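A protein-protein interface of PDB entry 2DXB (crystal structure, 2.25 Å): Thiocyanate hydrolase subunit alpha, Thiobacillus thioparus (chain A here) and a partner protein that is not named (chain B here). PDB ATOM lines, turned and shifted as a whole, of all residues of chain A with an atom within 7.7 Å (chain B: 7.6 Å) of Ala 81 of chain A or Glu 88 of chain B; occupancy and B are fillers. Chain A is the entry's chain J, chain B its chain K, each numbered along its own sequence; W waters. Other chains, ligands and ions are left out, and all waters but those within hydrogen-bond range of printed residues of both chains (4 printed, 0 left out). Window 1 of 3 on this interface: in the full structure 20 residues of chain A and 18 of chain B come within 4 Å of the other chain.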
ATOM      1  N   PHE A  52      26.938  -3.264 -29.777  1.00  0.00           N
ATOM      2  CA  PHE A  52      26.447  -1.983 -29.262  1.00  0.00           C
ATOM      3  C   PHE A  52      27.345  -0.763 -29.441  1.00  0.00           C
ATOM      4  O   PHE A  52      26.855   0.320 -29.757  1.00  0.00           O
ATOM      5  CB  PHE A  52      26.054  -2.112 -27.781  1.00  0.00           C
ATOM      6  CG  PHE A  52      25.034  -3.187 -27.517  1.00  0.00           C
ATOM      7  CD1 PHE A  52      24.006  -3.430 -28.430  1.00  0.00           C
ATOM      8  CD2 PHE A  52      25.096  -3.957 -26.357  1.00  0.00           C
ATOM      9  CE1 PHE A  52      23.052  -4.426 -28.196  1.00  0.00           C
ATOM     10  CE2 PHE A  52      24.147  -4.960 -26.108  1.00  0.00           C
ATOM     11  CZ  PHE A  52      23.120  -5.194 -27.034  1.00  0.00           C
ATOM     12  N   TYR A  53      28.649  -0.909 -29.241  1.00  0.00           N
ATOM     13  CA  TYR A  53      29.521   0.244 -29.404  1.00  0.00           C
ATOM     14  C   TYR A  53      31.008  -0.051 -29.370  1.00  0.00           C
ATOM     15  O   TYR A  53      31.463  -0.940 -28.657  1.00  0.00           O
ATOM     16  CB  TYR A  53      29.207   1.289 -28.332  1.00  0.00           C
ATOM     17  CG  TYR A  53      29.798   2.655 -28.613  1.00  0.00           C
ATOM     18  CD1 TYR A  53      29.422   3.376 -29.751  1.00  0.00           C
ATOM     19  CD2 TYR A  53      30.713   3.238 -27.738  1.00  0.00           C
ATOM     20  CE1 TYR A  53      29.937   4.643 -30.004  1.00  0.00           C
ATOM     21  CE2 TYR A  53      31.235   4.511 -27.982  1.00  0.00           C
ATOM     22  CZ  TYR A  53      30.839   5.205 -29.117  1.00  0.00           C
ATOM     23  OH  TYR A  53      31.324   6.468 -29.362  1.00  0.00           O
ATOM     24  N   THR A  54      31.754   0.715 -30.157  1.00  0.00           N
ATOM     25  CA  THR A  54      33.204   0.605 -30.220  1.00  0.00           C
ATOM     26  C   THR A  54      33.743   1.765 -31.040  1.00  0.00           C
ATOM     27  O   THR A  54      33.050   2.285 -31.920  1.00  0.00           O
ATOM     28  CB  THR A  54      33.667  -0.714 -30.889  1.00  0.00           C
ATOM     29  OG1 THR A  54      35.099  -0.725 -30.972  1.00  0.00           O
ATOM     30  CG2 THR A  54      33.098  -0.840 -32.294  1.00  0.00           C
ATOM     31  N   ARG A  55      34.967   2.184 -30.739  1.00  0.00           N
ATOM     32  CA  ARG A  55      35.596   3.256 -31.495  1.00  0.00           C
ATOM     33  C   ARG A  55      36.909   2.756 -32.099  1.00  0.00           C
ATOM     34  O   ARG A  55      37.772   3.540 -32.502  1.00  0.00           O
ATOM     35  CB  ARG A  55      35.819   4.495 -30.622  1.00  0.00           C
ATOM     36  CG  ARG A  55      34.500   5.186 -30.229  1.00  0.00           C
ATOM     37  CD  ARG A  55      34.707   6.593 -29.689  1.00  0.00           C
ATOM     38  NE  ARG A  55      35.014   7.562 -30.740  1.00  0.00           N
ATOM     39  CZ  ARG A  55      34.125   8.053 -31.598  1.00  0.00           C
ATOM     40  NH1 ARG A  55      32.847   7.672 -31.545  1.00  0.00           N
ATOM     41  NH2 ARG A  55      34.511   8.933 -32.510  1.00  0.00           N
ATOM     42  N   SER A  74      42.533   7.813 -20.235  1.00  0.00           N
ATOM     43  CA  SER A  74      41.108   8.081 -20.228  1.00  0.00           C
ATOM     44  C   SER A  74      40.305   6.798 -20.202  1.00  0.00           C
ATOM     45  O   SER A  74      40.827   5.719 -20.484  1.00  0.00           O
ATOM     46  CB  SER A  74      40.738   8.880 -21.488  1.00  0.00           C
ATOM     47  OG  SER A  74      39.342   8.858 -21.743  1.00  0.00           O
ATOM     48  N   PRO A  75      39.024   6.894 -19.820  1.00  0.00           N
ATOM     49  CA  PRO A  75      38.183   5.696 -19.797  1.00  0.00           C
ATOM     50  C   PRO A  75      38.017   5.320 -21.272  1.00  0.00           C
ATOM     51  O   PRO A  75      38.045   6.197 -22.133  1.00  0.00           O
ATOM     52  CB  PRO A  75      36.872   6.206 -19.206  1.00  0.00           C
ATOM     53  CG  PRO A  75      37.307   7.322 -18.311  1.00  0.00           C
ATOM     54  CD  PRO A  75      38.358   8.023 -19.144  1.00  0.00           C
ATOM     55  N   ALA A  76      37.868   4.039 -21.581  1.00  0.00           N
ATOM     56  CA  ALA A  76      37.679   3.656 -22.972  1.00  0.00           C
ATOM     57  C   ALA A  76      36.308   4.197 -23.378  1.00  0.00           C
ATOM     58  O   ALA A  76      35.433   4.372 -22.527  1.00  0.00           O
ATOM     59  CB  ALA A  76      37.717   2.145 -23.117  1.00  0.00           C
ATOM     60  N   ALA A  77      36.121   4.474 -24.665  1.00  0.00           N
ATOM     61  CA  ALA A  77      34.839   4.997 -25.137  1.00  0.00           C
ATOM     62  C   ALA A  77      33.730   3.981 -24.859  1.00  0.00           C
ATOM     63  O   ALA A  77      32.589   4.348 -24.590  1.00  0.00           O
ATOM     64  CB  ALA A  77      34.914   5.311 -26.631  1.00  0.00           C
ATOM     65  N   GLU A  78      34.081   2.702 -24.911  1.00  0.00           N
ATOM     66  CA  GLU A  78      33.129   1.627 -24.662  1.00  0.00           C
ATOM     67  C   GLU A  78      32.473   1.780 -23.283  1.00  0.00           C
ATOM     68  O   GLU A  78      31.325   1.378 -23.086  1.00  0.00           O
ATOM     69  CB  GLU A  78      33.835   0.270 -24.750  1.00  0.00           C
ATOM     70  CG  GLU A  78      34.409  -0.099 -26.126  1.00  0.00           C
ATOM     71  CD  GLU A  78      35.518   0.837 -26.604  1.00  0.00           C
ATOM     72  OE1 GLU A  78      36.140   1.523 -25.767  1.00  0.00           O
ATOM     73  OE2 GLU A  78      35.782   0.872 -27.825  1.00  0.00           O
ATOM     74  N   ASP A  79      33.201   2.359 -22.331  1.00  0.00           N
ATOM     75  CA  ASP A  79      32.659   2.554 -20.988  1.00  0.00           C
ATOM     76  C   ASP A  79      32.084   3.956 -20.809  1.00  0.00           C
ATOM     77  O   ASP A  79      30.988   4.129 -20.273  1.00  0.00           O
ATOM     78  CB  ASP A  79      33.739   2.305 -19.925  1.00  0.00           C
ATOM     79  CG  ASP A  79      34.109   0.838 -19.801  1.00  0.00           C
ATOM     80  OD1 ASP A  79      33.190  -0.012 -19.855  1.00  0.00           O
ATOM     81  OD2 ASP A  79      35.312   0.530 -19.637  1.00  0.00           O
ATOM     82  N   GLU A  80      32.824   4.958 -21.267  1.00  0.00           N
ATOM     83  CA  GLU A  80      32.392   6.343 -21.140  1.00  0.00           C
ATOM     84  C   GLU A  80      31.051   6.596 -21.833  1.00  0.00           C
ATOM     85  O   GLU A  80      30.224   7.358 -21.331  1.00  0.00           O
ATOM     86  CB  GLU A  80      33.471   7.272 -21.709  1.00  0.00           C
ATOM     87  CG  GLU A  80      33.312   8.742 -21.342  1.00  0.00           C
ATOM     88  CD  GLU A  80      34.575   9.552 -21.627  1.00  0.00           C
ATOM     89  OE1 GLU A  80      35.069   9.509 -22.777  1.00  0.00           O
ATOM     90  OE2 GLU A  80      35.073  10.232 -20.700  1.00  0.00           O
ATOM     91  N   ALA A  81      30.832   5.946 -22.973  1.00  0.00           N
ATOM     92  CA  ALA A  81      29.592   6.123 -23.731  1.00  0.00           C
ATOM     93  C   ALA A  81      28.373   5.563 -23.005  1.00  0.00           C
ATOM     94  O   ALA A  81      27.239   5.752 -23.447  1.00  0.00           O
ATOM     95  CB  ALA A  81      29.721   5.474 -25.112  1.00  0.00           C
ATOM     96  N   PHE A  82      28.611   4.869 -21.898  1.00  0.00           N
ATOM     97  CA  PHE A  82      27.529   4.295 -21.112  1.00  0.00           C
ATOM     98  C   PHE A  82      27.575   4.772 -19.661  1.00  0.00           C
ATOM     99  O   PHE A  82      26.994   4.153 -18.771  1.00  0.00           O
ATOM    100  CB  PHE A  82      27.574   2.766 -21.194  1.00  0.00           C
ATOM    101  CG  PHE A  82      27.057   2.226 -22.498  1.00  0.00           C
ATOM    102  CD1 PHE A  82      25.690   2.167 -22.744  1.00  0.00           C
ATOM    103  CD2 PHE A  82      27.933   1.845 -23.505  1.00  0.00           C
ATOM    104  CE1 PHE A  82      25.203   1.742 -23.977  1.00  0.00           C
ATOM    105  CE2 PHE A  82      27.458   1.419 -24.742  1.00  0.00           C
ATOM    106  CZ  PHE A  82      26.092   1.369 -24.979  1.00  0.00           C
ATOM    107  N   GLY A  83      28.270   5.887 -19.445  1.00  0.00           N
ATOM    108  CA  GLY A  83      28.373   6.476 -18.121  1.00  0.00           C
ATOM    109  C   GLY A  83      29.252   5.760 -17.117  1.00  0.00           C
ATOM    110  O   GLY A  83      29.169   6.032 -15.921  1.00  0.00           O
ATOM    111  N   ASN A  84      30.102   4.856 -17.590  1.00  0.00           N
ATOM    112  CA  ASN A  84      30.982   4.102 -16.701  1.00  0.00           C
ATOM    113  C   ASN A  84      32.415   4.618 -16.833  1.00  0.00           C
ATOM    114  O   ASN A  84      33.125   4.258 -17.766  1.00  0.00           O
ATOM    115  CB  ASN A  84      30.905   2.624 -17.069  1.00  0.00           C
ATOM    116  CG  ASN A  84      29.474   2.098 -17.070  1.00  0.00           C
ATOM    117  OD1 ASN A  84      29.070   1.353 -17.970  1.00  0.00           O
ATOM    118  ND2 ASN A  84      28.701   2.479 -16.058  1.00  0.00           N
ATOM    119  N   GLU A  85      32.836   5.460 -15.895  1.00  0.00           N
ATOM    120  CA  GLU A  85      34.171   6.051 -15.939  1.00  0.00           C
ATOM    121  C   GLU A  85      35.113   5.623 -14.815  1.00  0.00           C
ATOM    122  O   GLU A  85      36.160   6.239 -14.615  1.00  0.00           O
ATOM    123  CB  GLU A  85      34.051   7.580 -15.935  1.00  0.00           C
ATOM    124  CG  GLU A  85      33.460   8.168 -17.215  1.00  0.00           C
ATOM    125  CD  GLU A  85      33.183   9.662 -17.108  1.00  0.00           C
ATOM    126  OE1 GLU A  85      33.985  10.381 -16.474  1.00  0.00           O
ATOM    127  OE2 GLU A  85      32.165  10.123 -17.669  1.00  0.00           O
ATOM    128  N   HIS B  48      28.221   3.719 -37.329  1.00  0.00           N
ATOM    129  CA  HIS B  48      29.208   4.743 -37.669  1.00  0.00           C
ATOM    130  C   HIS B  48      30.542   4.255 -38.230  1.00  0.00           C
ATOM    131  O   HIS B  48      31.308   5.051 -38.777  1.00  0.00           O
ATOM    132  CB  HIS B  48      29.475   5.646 -36.455  1.00  0.00           C
ATOM    133  CG  HIS B  48      30.198   4.968 -35.328  1.00  0.00           C
ATOM    134  ND1 HIS B  48      30.554   5.630 -34.173  1.00  0.00           N
ATOM    135  CD2 HIS B  48      30.618   3.687 -35.174  1.00  0.00           C
ATOM    136  CE1 HIS B  48      31.163   4.788 -33.354  1.00  0.00           C
ATOM    137  NE2 HIS B  48      31.215   3.604 -33.937  1.00  0.00           N
ATOM    138  N   ALA B  80      25.815  18.947 -22.630  1.00  0.00           N
ATOM    139  CA  ALA B  80      27.030  18.271 -22.188  1.00  0.00           C
ATOM    140  C   ALA B  80      27.709  19.154 -21.156  1.00  0.00           C
ATOM    141  O   ALA B  80      28.177  18.685 -20.120  1.00  0.00           O
ATOM    142  CB  ALA B  80      27.961  18.034 -23.366  1.00  0.00           C
ATOM    143  N   TRP B  85      24.900  14.772 -20.267  1.00  0.00           N
ATOM    144  CA  TRP B  85      25.631  13.694 -20.926  1.00  0.00           C
ATOM    145  C   TRP B  85      27.024  14.146 -21.336  1.00  0.00           C
ATOM    146  O   TRP B  85      27.318  15.342 -21.355  1.00  0.00           O
ATOM    147  CB  TRP B  85      24.886  13.185 -22.171  1.00  0.00           C
ATOM    148  CG  TRP B  85      24.664  14.208 -23.281  1.00  0.00           C
ATOM    149  CD1 TRP B  85      25.095  15.510 -23.318  1.00  0.00           C
ATOM    150  CD2 TRP B  85      23.924  14.000 -24.493  1.00  0.00           C
ATOM    151  NE1 TRP B  85      24.664  16.122 -24.474  1.00  0.00           N
ATOM    152  CE2 TRP B  85      23.943  15.220 -25.212  1.00  0.00           C
ATOM    153  CE3 TRP B  85      23.243  12.902 -25.041  1.00  0.00           C
ATOM    154  CZ2 TRP B  85      23.306  15.371 -26.455  1.00  0.00           C
ATOM    155  CZ3 TRP B  85      22.609  13.052 -26.279  1.00  0.00           C
ATOM    156  CH2 TRP B  85      22.646  14.280 -26.969  1.00  0.00           C
ATOM    157  N   THR B  86      27.888  13.182 -21.633  1.00  0.00           N
ATOM    158  CA  THR B  86      29.232  13.486 -22.107  1.00  0.00           C
ATOM    159  C   THR B  86      29.133  13.367 -23.630  1.00  0.00           C
ATOM    160  O   THR B  86      28.156  12.814 -24.145  1.00  0.00           O
ATOM    161  CB  THR B  86      30.264  12.475 -21.584  1.00  0.00           C
ATOM    162  OG1 THR B  86      29.830  11.146 -21.900  1.00  0.00           O
ATOM    163  CG2 THR B  86      30.432  12.618 -20.074  1.00  0.00           C
ATOM    164  N   ALA B  87      30.121  13.879 -24.354  1.00  0.00           N
ATOM    165  CA  ALA B  87      30.077  13.799 -25.812  1.00  0.00           C
ATOM    166  C   ALA B  87      30.064  12.345 -26.286  1.00  0.00           C
ATOM    167  O   ALA B  87      29.458  12.027 -27.310  1.00  0.00           O
ATOM    168  CB  ALA B  87      31.260  14.543 -26.425  1.00  0.00           C
ATOM    169  N   GLU B  88      30.724  11.460 -25.545  1.00  0.00           N
ATOM    170  CA  GLU B  88      30.748  10.055 -25.930  1.00  0.00           C
ATOM    171  C   GLU B  88      29.372   9.409 -25.846  1.00  0.00           C
ATOM    172  O   GLU B  88      29.021   8.582 -26.692  1.00  0.00           O
ATOM    173  CB  GLU B  88      31.755   9.271 -25.086  1.00  0.00           C
ATOM    174  CG  GLU B  88      33.101   9.171 -25.769  1.00  0.00           C
ATOM    175  CD  GLU B  88      32.968   8.614 -27.178  1.00  0.00           C
ATOM    176  OE1 GLU B  88      33.463   9.256 -28.133  1.00  0.00           O
ATOM    177  OE2 GLU B  88      32.358   7.533 -27.324  1.00  0.00           O
ATOM    178  N   GLU B  89      28.591   9.778 -24.834  1.00  0.00           N
ATOM    179  CA  GLU B  89      27.245   9.234 -24.714  1.00  0.00           C
ATOM    180  C   GLU B  89      26.454   9.735 -25.922  1.00  0.00           C
ATOM    181  O   GLU B  89      25.704   8.979 -26.540  1.00  0.00           O
ATOM    182  CB  GLU B  89      26.578   9.685 -23.406  1.00  0.00           C
ATOM    183  CG  GLU B  89      27.190   9.058 -22.158  1.00  0.00           C
ATOM    184  CD  GLU B  89      26.511   9.494 -20.862  1.00  0.00           C
ATOM    185  OE1 GLU B  89      26.552  10.696 -20.535  1.00  0.00           O
ATOM    186  OE2 GLU B  89      25.940   8.631 -20.166  1.00  0.00           O
ATOM    187  N   ARG B  90      26.636  11.006 -26.281  1.00  0.00           N
ATOM    188  CA  ARG B  90      25.918  11.542 -27.434  1.00  0.00           C
ATOM    189  C   ARG B  90      26.257  10.754 -28.699  1.00  0.00           C
ATOM    190  O   ARG B  90      25.359  10.305 -29.414  1.00  0.00           O
ATOM    191  CB  ARG B  90      26.238  13.024 -27.658  1.00  0.00           C
ATOM    192  CG  ARG B  90      25.545  13.609 -28.899  1.00  0.00           C
ATOM    193  CD  ARG B  90      25.793  15.111 -29.059  1.00  0.00           C
ATOM    194  NE  ARG B  90      27.217  15.425 -29.137  1.00  0.00           N
ATOM    195  CZ  ARG B  90      28.003  15.110 -30.164  1.00  0.00           C
ATOM    196  NH1 ARG B  90      27.506  14.477 -31.217  1.00  0.00           N
ATOM    197  NH2 ARG B  90      29.296  15.405 -30.124  1.00  0.00           N
ATOM    198  N   ARG B  91      27.549  10.571 -28.964  1.00  0.00           N
ATOM    199  CA  ARG B  91      27.976   9.847 -30.162  1.00  0.00           C
ATOM    200  C   ARG B  91      27.388   8.451 -30.259  1.00  0.00           C
ATOM    201  O   ARG B  91      26.943   8.034 -31.326  1.00  0.00           O
ATOM    202  CB  ARG B  91      29.506   9.758 -30.231  1.00  0.00           C
ATOM    203  CG  ARG B  91      30.192  11.106 -30.365  1.00  0.00           C
ATOM    204  CD  ARG B  91      31.664  10.986 -30.765  1.00  0.00           C
ATOM    205  NE  ARG B  91      32.284  12.310 -30.769  1.00  0.00           N
ATOM    206  CZ  ARG B  91      32.802  12.896 -29.696  1.00  0.00           C
ATOM    207  NH1 ARG B  91      32.799  12.267 -28.527  1.00  0.00           N
ATOM    208  NH2 ARG B  91      33.273  14.132 -29.781  1.00  0.00           N
ATOM    209  N   ARG B  92      27.382   7.727 -29.143  1.00  0.00           N
ATOM    210  CA  ARG B  92      26.859   6.367 -29.122  1.00  0.00           C
ATOM    211  C   ARG B  92      25.370   6.344 -29.464  1.00  0.00           C
ATOM    212  O   ARG B  92      24.910   5.516 -30.249  1.00  0.00           O
ATOM    213  CB  ARG B  92      27.111   5.741 -27.739  1.00  0.00           C
ATOM    214  CG  ARG B  92      26.583   4.314 -27.560  1.00  0.00           C
ATOM    215  CD  ARG B  92      25.206   4.300 -26.903  1.00  0.00           C
ATOM    216  NE  ARG B  92      25.249   4.841 -25.543  1.00  0.00           N
ATOM    217  CZ  ARG B  92      24.191   4.956 -24.742  1.00  0.00           C
ATOM    218  NH1 ARG B  92      22.991   4.565 -25.156  1.00  0.00           N
ATOM    219  NH2 ARG B  92      24.329   5.476 -23.531  1.00  0.00           N
ATOM    220  N   LYS B  93      24.622   7.268 -28.878  1.00  0.00           N
ATOM    221  CA  LYS B  93      23.186   7.345 -29.109  1.00  0.00           C
ATOM    222  C   LYS B  93      22.864   7.919 -30.486  1.00  0.00           C
ATOM    223  O   LYS B  93      21.979   7.436 -31.198  1.00  0.00           O
ATOM    224  CB  LYS B  93      22.541   8.223 -28.034  1.00  0.00           C
ATOM    225  CG  LYS B  93      22.681   7.674 -26.621  1.00  0.00           C
ATOM    226  CD  LYS B  93      22.165   8.672 -25.596  1.00  0.00           C
ATOM    227  CE  LYS B  93      20.673   8.925 -25.755  1.00  0.00           C
ATOM    228  NZ  LYS B  93      19.885   7.705 -25.434  1.00  0.00           N
ATOM    229  N   GLN B  94      23.610   8.947 -30.851  1.00  0.00           N
ATOM    230  CA  GLN B  94      23.415   9.659 -32.105  1.00  0.00           C
ATOM    231  C   GLN B  94      23.920   8.974 -33.371  1.00  0.00           C
ATOM    232  O   GLN B  94      23.234   8.984 -34.394  1.00  0.00           O
ATOM    233  CB  GLN B  94      24.063  11.039 -31.981  1.00  0.00           C
ATOM    234  CG  GLN B  94      24.050  11.885 -33.233  1.00  0.00           C
ATOM    235  CD  GLN B  94      24.953  13.090 -33.088  1.00  0.00           C
ATOM    236  OE1 GLN B  94      24.716  13.960 -32.246  1.00  0.00           O
ATOM    237  NE2 GLN B  94      26.010  13.138 -33.896  1.00  0.00           N
ATOM    238  N   ASN B  95      25.103   8.374 -33.300  1.00  0.00           N
ATOM    239  CA  ASN B  95      25.703   7.743 -34.471  1.00  0.00           C
ATOM    240  C   ASN B  95      25.622   6.221 -34.556  1.00  0.00           C
ATOM    241  O   ASN B  95      26.031   5.634 -35.561  1.00  0.00           O
ATOM    242  CB  ASN B  95      27.173   8.172 -34.579  1.00  0.00           C
ATOM    243  CG  ASN B  95      27.346   9.677 -34.534  1.00  0.00           C
ATOM    244  OD1 ASN B  95      26.563  10.421 -35.131  1.00  0.00           O
ATOM    245  ND2 ASN B  95      28.388  10.135 -33.841  1.00  0.00           N
ATOM    246  N   ASP B  97      23.107   4.096 -32.020  1.00  0.00           N
ATOM    247  CA  ASP B  97      21.785   3.692 -31.564  1.00  0.00           C
ATOM    248  C   ASP B  97      20.651   3.979 -32.550  1.00  0.00           C
ATOM    249  O   ASP B  97      19.651   3.266 -32.555  1.00  0.00           O
ATOM    250  CB  ASP B  97      21.463   4.352 -30.217  1.00  0.00           C
ATOM    251  CG  ASP B  97      22.173   3.684 -29.043  1.00  0.00           C
ATOM    252  OD1 ASP B  97      22.977   2.755 -29.263  1.00  0.00           O
ATOM    253  OD2 ASP B  97      21.923   4.096 -27.892  1.00  0.00           O
HETATM  254  O   HOH W   1      30.225   9.449 -19.755  1.00  0.00           O
HETATM  255  O   HOH W   2      24.486   1.227 -30.708  1.00  0.00           O
HETATM  256  O   HOH W   3      30.687   8.393 -33.524  1.00  0.00           O
HETATM  257  O   HOH W   4      33.351  12.215 -23.625  1.00  0.00           O
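Of the 16 printed residues of chain A, 9 touch a printed residue of chain B.
Printed residues of chain A that touch a printed residue of chain B: Tyr 53, Thr 54, Arg 55, Ala 77, Glu 80, Ala 81, Phe 82, Gly 83 and Glu 85.
Hydrophobic or aromatic side chains of chain B within 4 Å of the printed part of chain A: His 48.
Among the printed residues, Asp or Glu carboxylates within 4 Å of a Lys or Arg side-chain nitrogen of the other chain: Arg 55 of chain A with Glu 88 of chain B.
Printed residues of chain B within 4 Å of Tyr 53 of chain A: His 48 (3.6 Å), Glu 88 (2.5 Å), Arg 91 (3.9 Å) and Arg 92 (3.6 Å).
Of the printed residues of chain B, Arg 55 of chain A touches His 48 (3.8 Å), Glu 88 (3.3 Å) and Arg 91 (3.6 Å).
Ala 81 of chain A touches just these residues of chain B: Glu 88, Glu 89 and Arg 92.
Printed residues of chain B within 4 Å of Gly 83 of chain A: Glu 89 (3.7 Å).
Printed residues of chain A within 4 Å of Thr 86 of chain B: Glu 80 (3.9 Å) and Glu 85 (3.9 Å).
No residue of chain A comes within 4 Å of Ala 87 of chain B.
Glu 88 of chain B touches five residues of chain A.
Printed residues of chain A within 4 Å of Arg 91 of chain B: Tyr 53 and Arg 55.
The nearest residue of chain B that does not touch Ala 81 of chain A is Thr 86 of chain B (5.4 Å).
The nearest residue of chain A that does not touch Glu 88 of chain B is Glu 78 of chain A (5.7 Å).
Water W2 lies within hydrogen-bond range of OD1 of Asp 97 of chain B and O of Phe 52 of chain A.
Water W1 lies within hydrogen-bond range of the backbone carbonyl oxygen (O) of Glu 80 of chain A (2.6 Å), the side-chain hydroxyl (OG1) of Thr 86 of chain B (2.8 Å) and the side-chain carboxylate (OE2) of Glu 85 of chain A (2.9 Å).
Water W3 lies within hydrogen-bond range of ND1 of His 48 of chain B, ND2 of Asn 95 of chain B and NH1 of Arg 55 of chain A.
Water W4 bridges OE1 of Glu 80 of chain A (3.3 Å) and N of Glu 88 of chain B (3.3 Å).
The side-chain carboxylate of Glu 88 of chain B is in salt-bridge range of the guanidinium group of Arg 55 of chain A (3.5 Å).
The backbone carbonyl oxygen of Ala 81 of chain A is in hydrogen-bond range of the guanidinium group of Arg 92 of chain B (2.9 Å).
The side-chain carboxylate of Glu 88 of chain B sits at hydrogen-bond distance from the side-chain hydroxyl of Tyr 53 of chain A.
A ring nitrogen (NE2) of His 48 of chain B lies within hydrogen-bond range of the backbone carbonyl oxygen (O) of Thr 54 of chain A (3.0 Å).
Tyr 53 of chain A touches His 48 of chain B.
CE1 of Tyr 53 of chain A touches CA of Arg 92 of chain B, 3.6 Å away.
Arg 55 of chain A touches His 48 of chain B.
Arg 55 of chain A touches Arg 91 of chain B.
Thr 86 of chain B touches Glu 80 of chain A (OG1 to O, 3.9 Å).
Glu 88 of chain B touches Glu 80 of chain A.
Glu 80 of chain A touches Glu 89 of chain B (O to CG, 3.6 Å).
Ala 81 of chain A touches Glu 88 of chain B (CB to O, 3.6 Å).
Arg 92 of chain B touches Phe 82 of chain A (CZ to CE1, 3.5 Å).
Glu 85 of chain A touches Thr 86 of chain B.
The side-chain carboxylate (OE1) of Glu 88 of chain B lies within salt-bridge range of the guanidinium group (NH1) of Arg 91 of chain B (3.1 Å).
The backbone NH (N) of Arg 55 of chain A sits at hydrogen-bond distance from the side-chain carboxylate (OE2) of Glu 78 of chain A, 3.3 Å away.
The side-chain carboxylate of Asp 97 of chain B lies within salt-bridge range of the guanidinium group of Arg 92 of chain B (3.0 Å).
The backbone NH (N) of His 48 of chain B lies within hydrogen-bond range of the backbone carbonyl oxygen (O) of Asn 95 of chain B.
The backbone NH (N) of Thr 86 of chain B sits at hydrogen-bond distance from the side-chain carboxylate (OE1) of Glu 89 of chain B.
The guanidinium group (NH1) of Arg 55 of chain A sits at hydrogen-bond distance from the side-chain hydroxyl (OH) of Tyr 53 of chain A (2.9 Å).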
